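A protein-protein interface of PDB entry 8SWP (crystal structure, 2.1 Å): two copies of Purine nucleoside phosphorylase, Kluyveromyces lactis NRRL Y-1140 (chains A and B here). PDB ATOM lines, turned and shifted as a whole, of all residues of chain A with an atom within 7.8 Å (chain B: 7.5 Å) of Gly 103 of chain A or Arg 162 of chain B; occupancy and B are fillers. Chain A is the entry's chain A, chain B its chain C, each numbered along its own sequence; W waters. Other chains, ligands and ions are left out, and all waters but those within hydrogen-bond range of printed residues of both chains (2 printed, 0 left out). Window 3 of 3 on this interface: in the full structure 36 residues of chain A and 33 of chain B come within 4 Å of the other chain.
OG1 of Thr 213 of chain A lies within hydrogen-bond range of NE2 of His 159 of chain B (2.8 Å). O of Ser 100 of chain A is in hydrogen-bond range of NH2 of Arg 162 of chain B, 3.1 Å away. The guanidinium group (NH2) of Arg 162 of chain B is in hydrogen-bond range of the backbone carbonyl oxygen (O) of His 104 of chain A (2.9 Å). The guanidinium group (NH1) of Arg 172 of chain B is in salt-bridge range of the side-chain carboxylate (OE2) of Glu 102 of chain A (2.9 Å). The backbone NH (N) of Gly 163 of chain B lies within hydrogen-bond range of the backbone carbonyl oxygen (O) of Tyr 101 of chain A (2.9 Å). A ring nitrogen (NE2) of His 210 of chain A is in hydrogen-bond range of the guanidinium group of Arg 162 of chain B (3.1 Å).
O of His 99 of chain A sits at hydrogen-bond distance from ND1 of His 104 of chain A (3.3 Å). O of Gly 163 of chain B lies within hydrogen-bond range of NH1 of Arg 172 of chain B, 2.6 Å away. O of Ser 100 of chain A sits at hydrogen-bond distance from NE2 of His 210 of chain A. OG of Ser 100 of chain A lies within hydrogen-bond range of O of His 104 of chain A (3.1 Å). ND1 of His 159 of chain B lies within hydrogen-bond range of N of Leu 161 of chain B, 3.0 Å away. The backbone NH (N) of Arg 172 of chain B lies close to the side-chain amide nitrogen (ND2) of Asn 165 of chain B, at 3.3 Å.
Among the printed residues, pairs that only touch across the chains: Phe 158 of chain A with Cys 156 of chain B (3.3 Å), Gly 211 of chain A with His 159 of chain B (3.3 Å), Pro 212 of chain A with Arg 172 of chain B (3.4 Å), His 210 of chain A with Gly 157 of chain B (3.5 Å), Glu 102 of chain A with Gly 163 of chain B (3.5 Å), Tyr 101 of chain A with Arg 172 of chain B (3.6 Å), Gly 103 of chain A with Arg 162 of chain B (3.6 Å), Tyr 101 of chain A with Arg 162 of chain B (3.7 Å), Glu 102 of chain A with Ala 164 of chain B (3.7 Å), Pro 212 of chain A with His 159 of chain B (3.8 Å), Pro 212 of chain A with Leu 161 of chain B (3.9 Å), Thr 213 of chain A with Leu 161 of chain B (3.9 Å), His 210 of chain A with Cys 156 of chain B (3.9 Å) and Gly 103 of chain A with Gly 163 of chain B (3.9 Å).
Leu 106 of chain A touches none of the printed residues of chain B. Of the printed residues of chain B, His 210 of chain A touches Cys 156 (3.9 Å), Gly 157 (3.5 Å) and Arg 162 (3.1 Å). Gly 163 of chain B touches just these residues of chain A: Tyr 101, Glu 102 and Gly 103. Phe 166 of chain B touches none of the printed residues of chain A. Printed residues of chain A within 4 Å of Arg 172 of chain B: Tyr 101, Glu 102 and Pro 212. The nearest residue of chain A that does not touch Arg 162 of chain B is Pro 212 of chain A (4.5 Å).
Of the 16 printed residues of chain B, 8 touch a printed residue of chain A. Along chain B the printed residues that touch a printed residue of chain A span positions 156 to 172. Of the 16 printed residues of chain A, 10 touch a printed residue of chain B. Printed residues of chain A that touch a printed residue of chain B: Ser 100, Tyr 101, Glu 102, Gly 103, His 104, Phe 158, His 210, Gly 211, Pro 212 and Thr 213. Among the printed residues, 20 pairs touch across the chains. Among the printed residues, Asp or Glu carboxylates within 4 Å of a Lys or Arg side-chain nitrogen of the other chain: Glu 102 of chain A with Arg 172 of chain B (2.9 Å).
Positions printed for both chains: 106 and 158.
Water W1 lies within hydrogen-bond range of N of Asn 165 of chain B (2.9 Å) and OE2 of Glu 102 of chain A (3.3 Å). Water W2 lies within hydrogen-bond range of the side-chain hydroxyl (OG1) of Thr 213 of chain A (3.1 Å) and a ring nitrogen (NE2) of His 159 of chain B (3.2 Å).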
ATOM      1  N   HIS A  99      21.215 -17.963  15.835  1.00  0.00           N
ATOM      2  CA  HIS A  99      20.480 -16.735  15.583  1.00  0.00           C
ATOM      3  C   HIS A  99      21.088 -15.592  16.384  1.00  0.00           C
ATOM      4  O   HIS A  99      21.628 -15.791  17.475  1.00  0.00           O
ATOM      5  CB  HIS A  99      19.003 -16.890  15.943  1.00  0.00           C
ATOM      6  CG  HIS A  99      18.258 -17.836  15.056  1.00  0.00           C
ATOM      7  ND1 HIS A  99      18.316 -19.204  15.211  1.00  0.00           N
ATOM      8  CD2 HIS A  99      17.444 -17.612  13.997  1.00  0.00           C
ATOM      9  CE1 HIS A  99      17.563 -19.782  14.292  1.00  0.00           C
ATOM     10  NE2 HIS A  99      17.024 -18.838  13.540  1.00  0.00           N
ATOM     11  N   SER A 100      20.988 -14.383  15.832  1.00  0.00           N
ATOM     12  CA  SER A 100      21.585 -13.237  16.500  1.00  0.00           C
ATOM     13  C   SER A 100      20.743 -12.745  17.668  1.00  0.00           C
ATOM     14  O   SER A 100      21.288 -12.154  18.608  1.00  0.00           O
ATOM     15  CB  SER A 100      21.814 -12.102  15.509  1.00  0.00           C
ATOM     16  OG  SER A 100      22.937 -11.346  15.914  1.00  0.00           O
ATOM     17  N   TYR A 101      19.429 -12.975  17.639  1.00  0.00           N
ATOM     18  CA  TYR A 101      18.602 -12.583  18.773  1.00  0.00           C
ATOM     19  C   TYR A 101      18.884 -13.413  20.017  1.00  0.00           C
ATOM     20  O   TYR A 101      18.386 -13.071  21.094  1.00  0.00           O
ATOM     21  CB  TYR A 101      17.112 -12.659  18.412  1.00  0.00           C
ATOM     22  CG  TYR A 101      16.630 -14.001  17.899  1.00  0.00           C
ATOM     23  CD1 TYR A 101      16.453 -15.080  18.760  1.00  0.00           C
ATOM     24  CD2 TYR A 101      16.326 -14.181  16.557  1.00  0.00           C
ATOM     25  CE1 TYR A 101      16.006 -16.300  18.294  1.00  0.00           C
ATOM     26  CE2 TYR A 101      15.874 -15.396  16.082  1.00  0.00           C
ATOM     27  CZ  TYR A 101      15.718 -16.453  16.953  1.00  0.00           C
ATOM     28  OH  TYR A 101      15.271 -17.666  16.485  1.00  0.00           O
ATOM     29  N   GLU A 102      19.660 -14.487  19.896  1.00  0.00           N
ATOM     30  CA  GLU A 102      20.080 -15.279  21.043  1.00  0.00           C
ATOM     31  C   GLU A 102      21.336 -14.729  21.706  1.00  0.00           C
ATOM     32  O   GLU A 102      21.775 -15.280  22.721  1.00  0.00           O
ATOM     33  CB  GLU A 102      20.313 -16.736  20.624  1.00  0.00           C
ATOM     34  CG  GLU A 102      19.056 -17.600  20.616  1.00  0.00           C
ATOM     35  CD  GLU A 102      18.425 -17.752  21.989  1.00  0.00           C
ATOM     36  OE1 GLU A 102      19.113 -17.502  23.002  1.00  0.00           O
ATOM     37  OE2 GLU A 102      17.231 -18.119  22.054  1.00  0.00           O
ATOM     38  N   GLY A 103      21.925 -13.667  21.160  1.00  0.00           N
ATOM     39  CA  GLY A 103      23.102 -13.041  21.730  1.00  0.00           C
ATOM     40  C   GLY A 103      24.387 -13.302  20.978  1.00  0.00           C
ATOM     41  O   GLY A 103      25.395 -12.643  21.266  1.00  0.00           O
ATOM     42  N   HIS A 104      24.393 -14.234  20.030  1.00  0.00           N
ATOM     43  CA  HIS A 104      25.603 -14.519  19.274  1.00  0.00           C
ATOM     44  C   HIS A 104      25.899 -13.395  18.286  1.00  0.00           C
ATOM     45  O   HIS A 104      24.993 -12.743  17.761  1.00  0.00           O
ATOM     46  CB  HIS A 104      25.471 -15.845  18.525  1.00  0.00           C
ATOM     47  CG  HIS A 104      25.028 -16.985  19.387  1.00  0.00           C
ATOM     48  ND1 HIS A 104      23.792 -17.582  19.255  1.00  0.00           N
ATOM     49  CD2 HIS A 104      25.655 -17.639  20.393  1.00  0.00           C
ATOM     50  CE1 HIS A 104      23.678 -18.553  20.142  1.00  0.00           C
ATOM     51  NE2 HIS A 104      24.795 -18.609  20.846  1.00  0.00           N
ATOM     52  N   SER A 105      27.186 -13.173  18.038  1.00  0.00           N
ATOM     53  CA  SER A 105      27.599 -12.192  17.051  1.00  0.00           C
ATOM     54  C   SER A 105      27.403 -12.747  15.643  1.00  0.00           C
ATOM     55  O   SER A 105      27.223 -13.951  15.440  1.00  0.00           O
ATOM     56  CB  SER A 105      29.061 -11.794  17.258  1.00  0.00           C
ATOM     57  OG  SER A 105      29.904 -12.933  17.246  1.00  0.00           O
ATOM     58  N   LEU A 106      27.433 -11.844  14.660  1.00  0.00           N
ATOM     59  CA  LEU A 106      27.294 -12.271  13.272  1.00  0.00           C
ATOM     60  C   LEU A 106      28.486 -13.111  12.833  1.00  0.00           C
ATOM     61  O   LEU A 106      28.333 -14.048  12.041  1.00  0.00           O
ATOM     62  CB  LEU A 106      27.125 -11.059  12.358  1.00  0.00           C
ATOM     63  CG  LEU A 106      25.764 -10.366  12.433  1.00  0.00           C
ATOM     64  CD1 LEU A 106      25.671  -9.236  11.419  1.00  0.00           C
ATOM     65  CD2 LEU A 106      24.645 -11.373  12.224  1.00  0.00           C
ATOM     66  N   GLU A 108      30.121 -15.233  14.643  1.00  0.00           N
ATOM     67  CA  GLU A 108      29.860 -16.591  15.104  1.00  0.00           C
ATOM     68  C   GLU A 108      28.782 -17.270  14.270  1.00  0.00           C
ATOM     69  O   GLU A 108      28.838 -18.487  14.062  1.00  0.00           O
ATOM     70  CB  GLU A 108      29.462 -16.582  16.581  1.00  0.00           C
ATOM     71  CG  GLU A 108      30.583 -16.180  17.529  1.00  0.00           C
ATOM     72  CD  GLU A 108      30.073 -15.575  18.822  1.00  0.00           C
ATOM     73  OE1 GLU A 108      28.878 -15.757  19.137  1.00  0.00           O
ATOM     74  OE2 GLU A 108      30.868 -14.917  19.527  1.00  0.00           O
ATOM     75  N   THR A 109      27.801 -16.505  13.783  1.00  0.00           N
ATOM     76  CA  THR A 109      26.720 -17.090  12.995  1.00  0.00           C
ATOM     77  C   THR A 109      27.230 -17.630  11.664  1.00  0.00           C
ATOM     78  O   THR A 109      26.833 -18.720  11.235  1.00  0.00           O
ATOM     79  CB  THR A 109      25.619 -16.053  12.765  1.00  0.00           C
ATOM     80  OG1 THR A 109      25.030 -15.689  14.020  1.00  0.00           O
ATOM     81  CG2 THR A 109      24.537 -16.606  11.845  1.00  0.00           C
ATOM     82  N   PHE A 158      25.065  -3.429  11.494  1.00  0.00           N
ATOM     83  CA  PHE A 158      24.992  -4.830  11.907  1.00  0.00           C
ATOM     84  C   PHE A 158      25.237  -5.696  10.675  1.00  0.00           C
ATOM     85  O   PHE A 158      24.320  -6.242  10.059  1.00  0.00           O
ATOM     86  CB  PHE A 158      23.643  -5.111  12.557  1.00  0.00           C
ATOM     87  CG  PHE A 158      23.559  -6.443  13.233  1.00  0.00           C
ATOM     88  CD1 PHE A 158      24.445  -6.783  14.240  1.00  0.00           C
ATOM     89  CD2 PHE A 158      22.579  -7.353  12.870  1.00  0.00           C
ATOM     90  CE1 PHE A 158      24.362  -8.006  14.867  1.00  0.00           C
ATOM     91  CE2 PHE A 158      22.493  -8.576  13.492  1.00  0.00           C
ATOM     92  CZ  PHE A 158      23.385  -8.900  14.493  1.00  0.00           C
ATOM     93  N   TYR A 208      15.555  -8.944   6.262  1.00  0.00           N
ATOM     94  CA  TYR A 208      16.115  -9.499   7.484  1.00  0.00           C
ATOM     95  C   TYR A 208      15.971  -8.481   8.609  1.00  0.00           C
ATOM     96  O   TYR A 208      16.460  -7.352   8.496  1.00  0.00           O
ATOM     97  CB  TYR A 208      17.581  -9.873   7.267  1.00  0.00           C
ATOM     98  CG  TYR A 208      18.377 -10.099   8.532  1.00  0.00           C
ATOM     99  CD1 TYR A 208      18.094 -11.165   9.376  1.00  0.00           C
ATOM    100  CD2 TYR A 208      19.424  -9.252   8.873  1.00  0.00           C
ATOM    101  CE1 TYR A 208      18.825 -11.374  10.530  1.00  0.00           C
ATOM    102  CE2 TYR A 208      20.161  -9.454  10.023  1.00  0.00           C
ATOM    103  CZ  TYR A 208      19.856 -10.516  10.849  1.00  0.00           C
ATOM    104  OH  TYR A 208      20.586 -10.724  11.996  1.00  0.00           O
ATOM    105  N   HIS A 210      16.221  -8.198  13.081  1.00  0.00           N
ATOM    106  CA  HIS A 210      16.980  -8.855  14.139  1.00  0.00           C
ATOM    107  C   HIS A 210      16.099  -9.760  14.991  1.00  0.00           C
ATOM    108  O   HIS A 210      16.504 -10.874  15.344  1.00  0.00           O
ATOM    109  CB  HIS A 210      17.671  -7.811  15.013  1.00  0.00           C
ATOM    110  CG  HIS A 210      18.518  -8.400  16.096  1.00  0.00           C
ATOM    111  ND1 HIS A 210      18.044  -8.623  17.371  1.00  0.00           N
ATOM    112  CD2 HIS A 210      19.805  -8.822  16.093  1.00  0.00           C
ATOM    113  CE1 HIS A 210      19.004  -9.153  18.109  1.00  0.00           C
ATOM    114  NE2 HIS A 210      20.083  -9.283  17.357  1.00  0.00           N
ATOM    115  N   GLY A 211      14.897  -9.305  15.333  1.00  0.00           N
ATOM    116  CA  GLY A 211      14.058 -10.022  16.263  1.00  0.00           C
ATOM    117  C   GLY A 211      14.445  -9.699  17.692  1.00  0.00           C
ATOM    118  O   GLY A 211      15.201  -8.758  17.950  1.00  0.00           O
ATOM    119  N   PRO A 212      13.947 -10.487  18.658  1.00  0.00           N
ATOM    120  CA  PRO A 212      13.081 -11.656  18.493  1.00  0.00           C
ATOM    121  C   PRO A 212      11.592 -11.324  18.529  1.00  0.00           C
ATOM    122  O   PRO A 212      10.764 -12.235  18.573  1.00  0.00           O
ATOM    123  CB  PRO A 212      13.467 -12.525  19.688  1.00  0.00           C
ATOM    124  CG  PRO A 212      13.756 -11.520  20.761  1.00  0.00           C
ATOM    125  CD  PRO A 212      14.342 -10.303  20.067  1.00  0.00           C
ATOM    126  N   THR A 213      11.255 -10.038  18.523  1.00  0.00           N
ATOM    127  CA  THR A 213       9.858  -9.635  18.509  1.00  0.00           C
ATOM    128  C   THR A 213       9.278  -9.755  17.108  1.00  0.00           C
ATOM    129  O   THR A 213       9.967  -9.546  16.106  1.00  0.00           O
ATOM    130  CB  THR A 213       9.692  -8.196  19.002  1.00  0.00           C
ATOM    131  OG1 THR A 213      10.675  -7.355  18.385  1.00  0.00           O
ATOM    132  CG2 THR A 213       9.830  -8.127  20.513  1.00  0.00           C
ATOM    133  N   GLN B  10      22.039 -11.998  35.739  1.00  0.00           N
ATOM    134  CA  GLN B  10      20.933 -11.065  35.555  1.00  0.00           C
ATOM    135  C   GLN B  10      19.706 -11.507  36.342  1.00  0.00           C
ATOM    136  O   GLN B  10      18.988 -10.674  36.908  1.00  0.00           O
ATOM    137  CB  GLN B  10      20.595 -10.935  34.070  1.00  0.00           C
ATOM    138  CG  GLN B  10      21.579 -10.095  33.274  1.00  0.00           C
ATOM    139  CD  GLN B  10      21.125  -9.874  31.844  1.00  0.00           C
ATOM    140  OE1 GLN B  10      20.033  -9.361  31.599  1.00  0.00           O
ATOM    141  NE2 GLN B  10      21.963 -10.263  30.890  1.00  0.00           N
ATOM    142  N   LEU B 106      20.642  -2.233  26.979  1.00  0.00           N
ATOM    143  CA  LEU B 106      19.210  -2.099  27.208  1.00  0.00           C
ATOM    144  C   LEU B 106      18.765  -2.959  28.386  1.00  0.00           C
ATOM    145  O   LEU B 106      17.718  -2.710  28.986  1.00  0.00           O
ATOM    146  CB  LEU B 106      18.427  -2.480  25.951  1.00  0.00           C
ATOM    147  CG  LEU B 106      18.173  -1.340  24.963  1.00  0.00           C
ATOM    148  CD1 LEU B 106      17.344  -1.814  23.781  1.00  0.00           C
ATOM    149  CD2 LEU B 106      17.506  -0.161  25.655  1.00  0.00           C
ATOM    150  N   ALA B 107      19.570  -3.974  28.710  1.00  0.00           N
ATOM    151  CA  ALA B 107      19.253  -4.838  29.843  1.00  0.00           C
ATOM    152  C   ALA B 107      19.246  -4.062  31.154  1.00  0.00           C
ATOM    153  O   ALA B 107      18.560  -4.456  32.105  1.00  0.00           O
ATOM    154  CB  ALA B 107      20.244  -5.999  29.915  1.00  0.00           C
ATOM    155  N   ARG B 114      11.427  -5.847  35.297  1.00  0.00           N
ATOM    156  CA  ARG B 114      11.390  -7.252  35.692  1.00  0.00           C
ATOM    157  C   ARG B 114      11.462  -7.412  37.205  1.00  0.00           C
ATOM    158  O   ARG B 114      10.857  -8.338  37.758  1.00  0.00           O
ATOM    159  CB  ARG B 114      12.527  -8.019  35.019  1.00  0.00           C
ATOM    160  CG  ARG B 114      12.397  -8.126  33.506  1.00  0.00           C
ATOM    161  CD  ARG B 114      13.258  -9.256  32.964  1.00  0.00           C
ATOM    162  NE  ARG B 114      13.488  -9.148  31.528  1.00  0.00           N
ATOM    163  CZ  ARG B 114      12.605  -9.487  30.598  1.00  0.00           C
ATOM    164  NH1 ARG B 114      11.404  -9.944  30.916  1.00  0.00           N
ATOM    165  NH2 ARG B 114      12.936  -9.367  29.315  1.00  0.00           N
ATOM    166  N   CYS B 156      17.374  -3.671  14.093  1.00  0.00           N
ATOM    167  CA  CYS B 156      18.798  -3.753  13.674  1.00  0.00           C
ATOM    168  C   CYS B 156      19.677  -4.500  14.680  1.00  0.00           C
ATOM    169  O   CYS B 156      20.719  -4.979  14.254  1.00  0.00           O
ATOM    170  CB  CYS B 156      19.355  -2.361  13.430  1.00  0.00           C
ATOM    171  SG  CYS B 156      18.441  -1.434  12.176  1.00  0.00           S
ATOM    172  N   GLY B 157      19.278  -4.628  15.942  1.00  0.00           N
ATOM    173  CA  GLY B 157      20.086  -5.423  16.889  1.00  0.00           C
ATOM    174  C   GLY B 157      20.109  -4.882  18.307  1.00  0.00           C
ATOM    175  O   GLY B 157      20.440  -5.652  19.204  1.00  0.00           O
ATOM    176  N   PHE B 158      19.803  -3.604  18.497  1.00  0.00           N
ATOM    177  CA  PHE B 158      19.710  -2.999  19.852  1.00  0.00           C
ATOM    178  C   PHE B 158      18.299  -3.275  20.383  1.00  0.00           C
ATOM    179  O   PHE B 158      17.425  -2.434  20.202  1.00  0.00           O
ATOM    180  CB  PHE B 158      20.075  -1.516  19.757  1.00  0.00           C
ATOM    181  CG  PHE B 158      20.217  -0.762  21.054  1.00  0.00           C
ATOM    182  CD1 PHE B 158      21.201  -1.096  21.969  1.00  0.00           C
ATOM    183  CD2 PHE B 158      19.394   0.315  21.336  1.00  0.00           C
ATOM    184  CE1 PHE B 158      21.342  -0.386  23.150  1.00  0.00           C
ATOM    185  CE2 PHE B 158      19.535   1.024  22.517  1.00  0.00           C
ATOM    186  CZ  PHE B 158      20.513   0.675  23.419  1.00  0.00           C
ATOM    187  N   HIS B 159      18.108  -4.420  21.028  1.00  0.00           N
ATOM    188  CA  HIS B 159      16.749  -4.845  21.449  1.00  0.00           C
ATOM    189  C   HIS B 159      16.746  -5.279  22.917  1.00  0.00           C
ATOM    190  O   HIS B 159      17.620  -6.039  23.339  1.00  0.00           O
ATOM    191  CB  HIS B 159      16.299  -5.997  20.546  1.00  0.00           C
ATOM    192  CG  HIS B 159      14.847  -6.305  20.547  1.00  0.00           C
ATOM    193  ND1 HIS B 159      14.198  -6.854  21.629  1.00  0.00           N
ATOM    194  CD2 HIS B 159      13.927  -6.160  19.594  1.00  0.00           C
ATOM    195  CE1 HIS B 159      12.922  -7.011  21.330  1.00  0.00           C
ATOM    196  NE2 HIS B 159      12.738  -6.600  20.098  1.00  0.00           N
ATOM    197  N   PRO B 160      15.735  -4.861  23.699  1.00  0.00           N
ATOM    198  CA  PRO B 160      15.647  -5.236  25.108  1.00  0.00           C
ATOM    199  C   PRO B 160      15.590  -6.753  25.351  1.00  0.00           C
ATOM    200  O   PRO B 160      16.007  -7.170  26.390  1.00  0.00           O
ATOM    201  CB  PRO B 160      14.326  -4.595  25.546  1.00  0.00           C
ATOM    202  CG  PRO B 160      13.557  -4.362  24.275  1.00  0.00           C
ATOM    203  CD  PRO B 160      14.625  -4.019  23.265  1.00  0.00           C
ATOM    204  N   LEU B 161      15.120  -7.523  24.369  1.00  0.00           N
ATOM    205  CA  LEU B 161      14.945  -8.986  24.567  1.00  0.00           C
ATOM    206  C   LEU B 161      16.088  -9.782  23.924  1.00  0.00           C
ATOM    207  O   LEU B 161      16.031 -11.013  23.963  1.00  0.00           O
ATOM    208  CB  LEU B 161      13.590  -9.408  23.993  1.00  0.00           C
ATOM    209  CG  LEU B 161      12.359  -8.707  24.559  1.00  0.00           C
ATOM    210  CD1 LEU B 161      11.093  -9.312  23.978  1.00  0.00           C
ATOM    211  CD2 LEU B 161      12.337  -8.793  26.075  1.00  0.00           C
ATOM    212  N   ARG B 162      17.095  -9.102  23.375  1.00  0.00           N
ATOM    213  CA  ARG B 162      18.255  -9.805  22.776  1.00  0.00           C
ATOM    214  C   ARG B 162      18.943 -10.641  23.854  1.00  0.00           C
ATOM    215  O   ARG B 162      19.035 -10.178  24.987  1.00  0.00           O
ATOM    216  CB  ARG B 162      19.225  -8.830  22.108  1.00  0.00           C
ATOM    217  CG  ARG B 162      20.457  -9.491  21.513  1.00  0.00           C
ATOM    218  CD  ARG B 162      21.381  -8.488  20.856  1.00  0.00           C
ATOM    219  NE  ARG B 162      22.093  -9.063  19.727  1.00  0.00           N
ATOM    220  CZ  ARG B 162      23.310  -9.580  19.798  1.00  0.00           C
ATOM    221  NH1 ARG B 162      24.075  -9.318  20.840  1.00  0.00           N
ATOM    222  NH2 ARG B 162      23.756 -10.356  18.826  1.00  0.00           N
ATOM    223  N   GLY B 163      19.413 -11.824  23.487  1.00  0.00           N
ATOM    224  CA  GLY B 163      20.038 -12.728  24.457  1.00  0.00           C
ATOM    225  C   GLY B 163      19.104 -13.848  24.858  1.00  0.00           C
ATOM    226  O   GLY B 163      18.001 -13.922  24.316  1.00  0.00           O
ATOM    227  N   ALA B 164      19.543 -14.684  25.788  1.00  0.00           N
ATOM    228  CA  ALA B 164      18.695 -15.781  26.293  1.00  0.00           C
ATOM    229  C   ALA B 164      17.383 -15.221  26.826  1.00  0.00           C
ATOM    230  O   ALA B 164      17.407 -14.209  27.531  1.00  0.00           O
ATOM    231  CB  ALA B 164      19.438 -16.541  27.347  1.00  0.00           C
ATOM    232  N   ASN B 165      16.283 -15.878  26.488  1.00  0.00           N
ATOM    233  CA  ASN B 165      14.949 -15.392  26.901  1.00  0.00           C
ATOM    234  C   ASN B 165      14.727 -15.640  28.391  1.00  0.00           C
ATOM    235  O   ASN B 165      15.204 -16.662  28.889  1.00  0.00           O
ATOM    236  CB  ASN B 165      13.829 -16.076  26.116  1.00  0.00           C
ATOM    237  CG  ASN B 165      12.454 -15.567  26.474  1.00  0.00           C
ATOM    238  OD1 ASN B 165      12.171 -14.388  26.310  1.00  0.00           O
ATOM    239  ND2 ASN B 165      11.597 -16.449  26.958  1.00  0.00           N
ATOM    240  N   PHE B 166      14.041 -14.722  29.060  1.00  0.00           N
ATOM    241  CA  PHE B 166      13.641 -14.948  30.468  1.00  0.00           C
ATOM    242  C   PHE B 166      12.333 -15.749  30.408  1.00  0.00           C
ATOM    243  O   PHE B 166      11.262 -15.135  30.344  1.00  0.00           O
ATOM    244  CB  PHE B 166      13.558 -13.600  31.186  1.00  0.00           C
ATOM    245  CG  PHE B 166      14.887 -12.969  31.506  1.00  0.00           C
ATOM    246  CD1 PHE B 166      15.570 -12.233  30.553  1.00  0.00           C
ATOM    247  CD2 PHE B 166      15.456 -13.112  32.759  1.00  0.00           C
ATOM    248  CE1 PHE B 166      16.794 -11.657  30.847  1.00  0.00           C
ATOM    249  CE2 PHE B 166      16.680 -12.535  33.052  1.00  0.00           C
ATOM    250  CZ  PHE B 166      17.346 -11.807  32.096  1.00  0.00           C
ATOM    251  N   ARG B 172       9.975 -16.439  24.055  1.00  0.00           N
ATOM    252  CA  ARG B 172      11.158 -16.125  23.218  1.00  0.00           C
ATOM    253  C   ARG B 172      10.749 -15.157  22.109  1.00  0.00           C
ATOM    254  O   ARG B 172      11.487 -14.202  21.857  1.00  0.00           O
ATOM    255  CB  ARG B 172      11.701 -17.406  22.584  1.00  0.00           C
ATOM    256  CG  ARG B 172      12.730 -17.182  21.488  1.00  0.00           C
ATOM    257  CD  ARG B 172      14.088 -16.832  22.055  1.00  0.00           C
ATOM    258  NE  ARG B 172      14.207 -15.409  22.304  1.00  0.00           N
ATOM    259  CZ  ARG B 172      15.270 -14.837  22.847  1.00  0.00           C
ATOM    260  NH1 ARG B 172      16.417 -15.486  22.882  1.00  0.00           N
ATOM    261  NH2 ARG B 172      15.182 -13.621  23.350  1.00  0.00           N
HETATM  262  O   HOH W   1      16.569 -18.425  25.224  1.00  0.00           O
HETATM  263  O   HOH W   2      10.561  -4.381  19.231  1.00  0.00           O
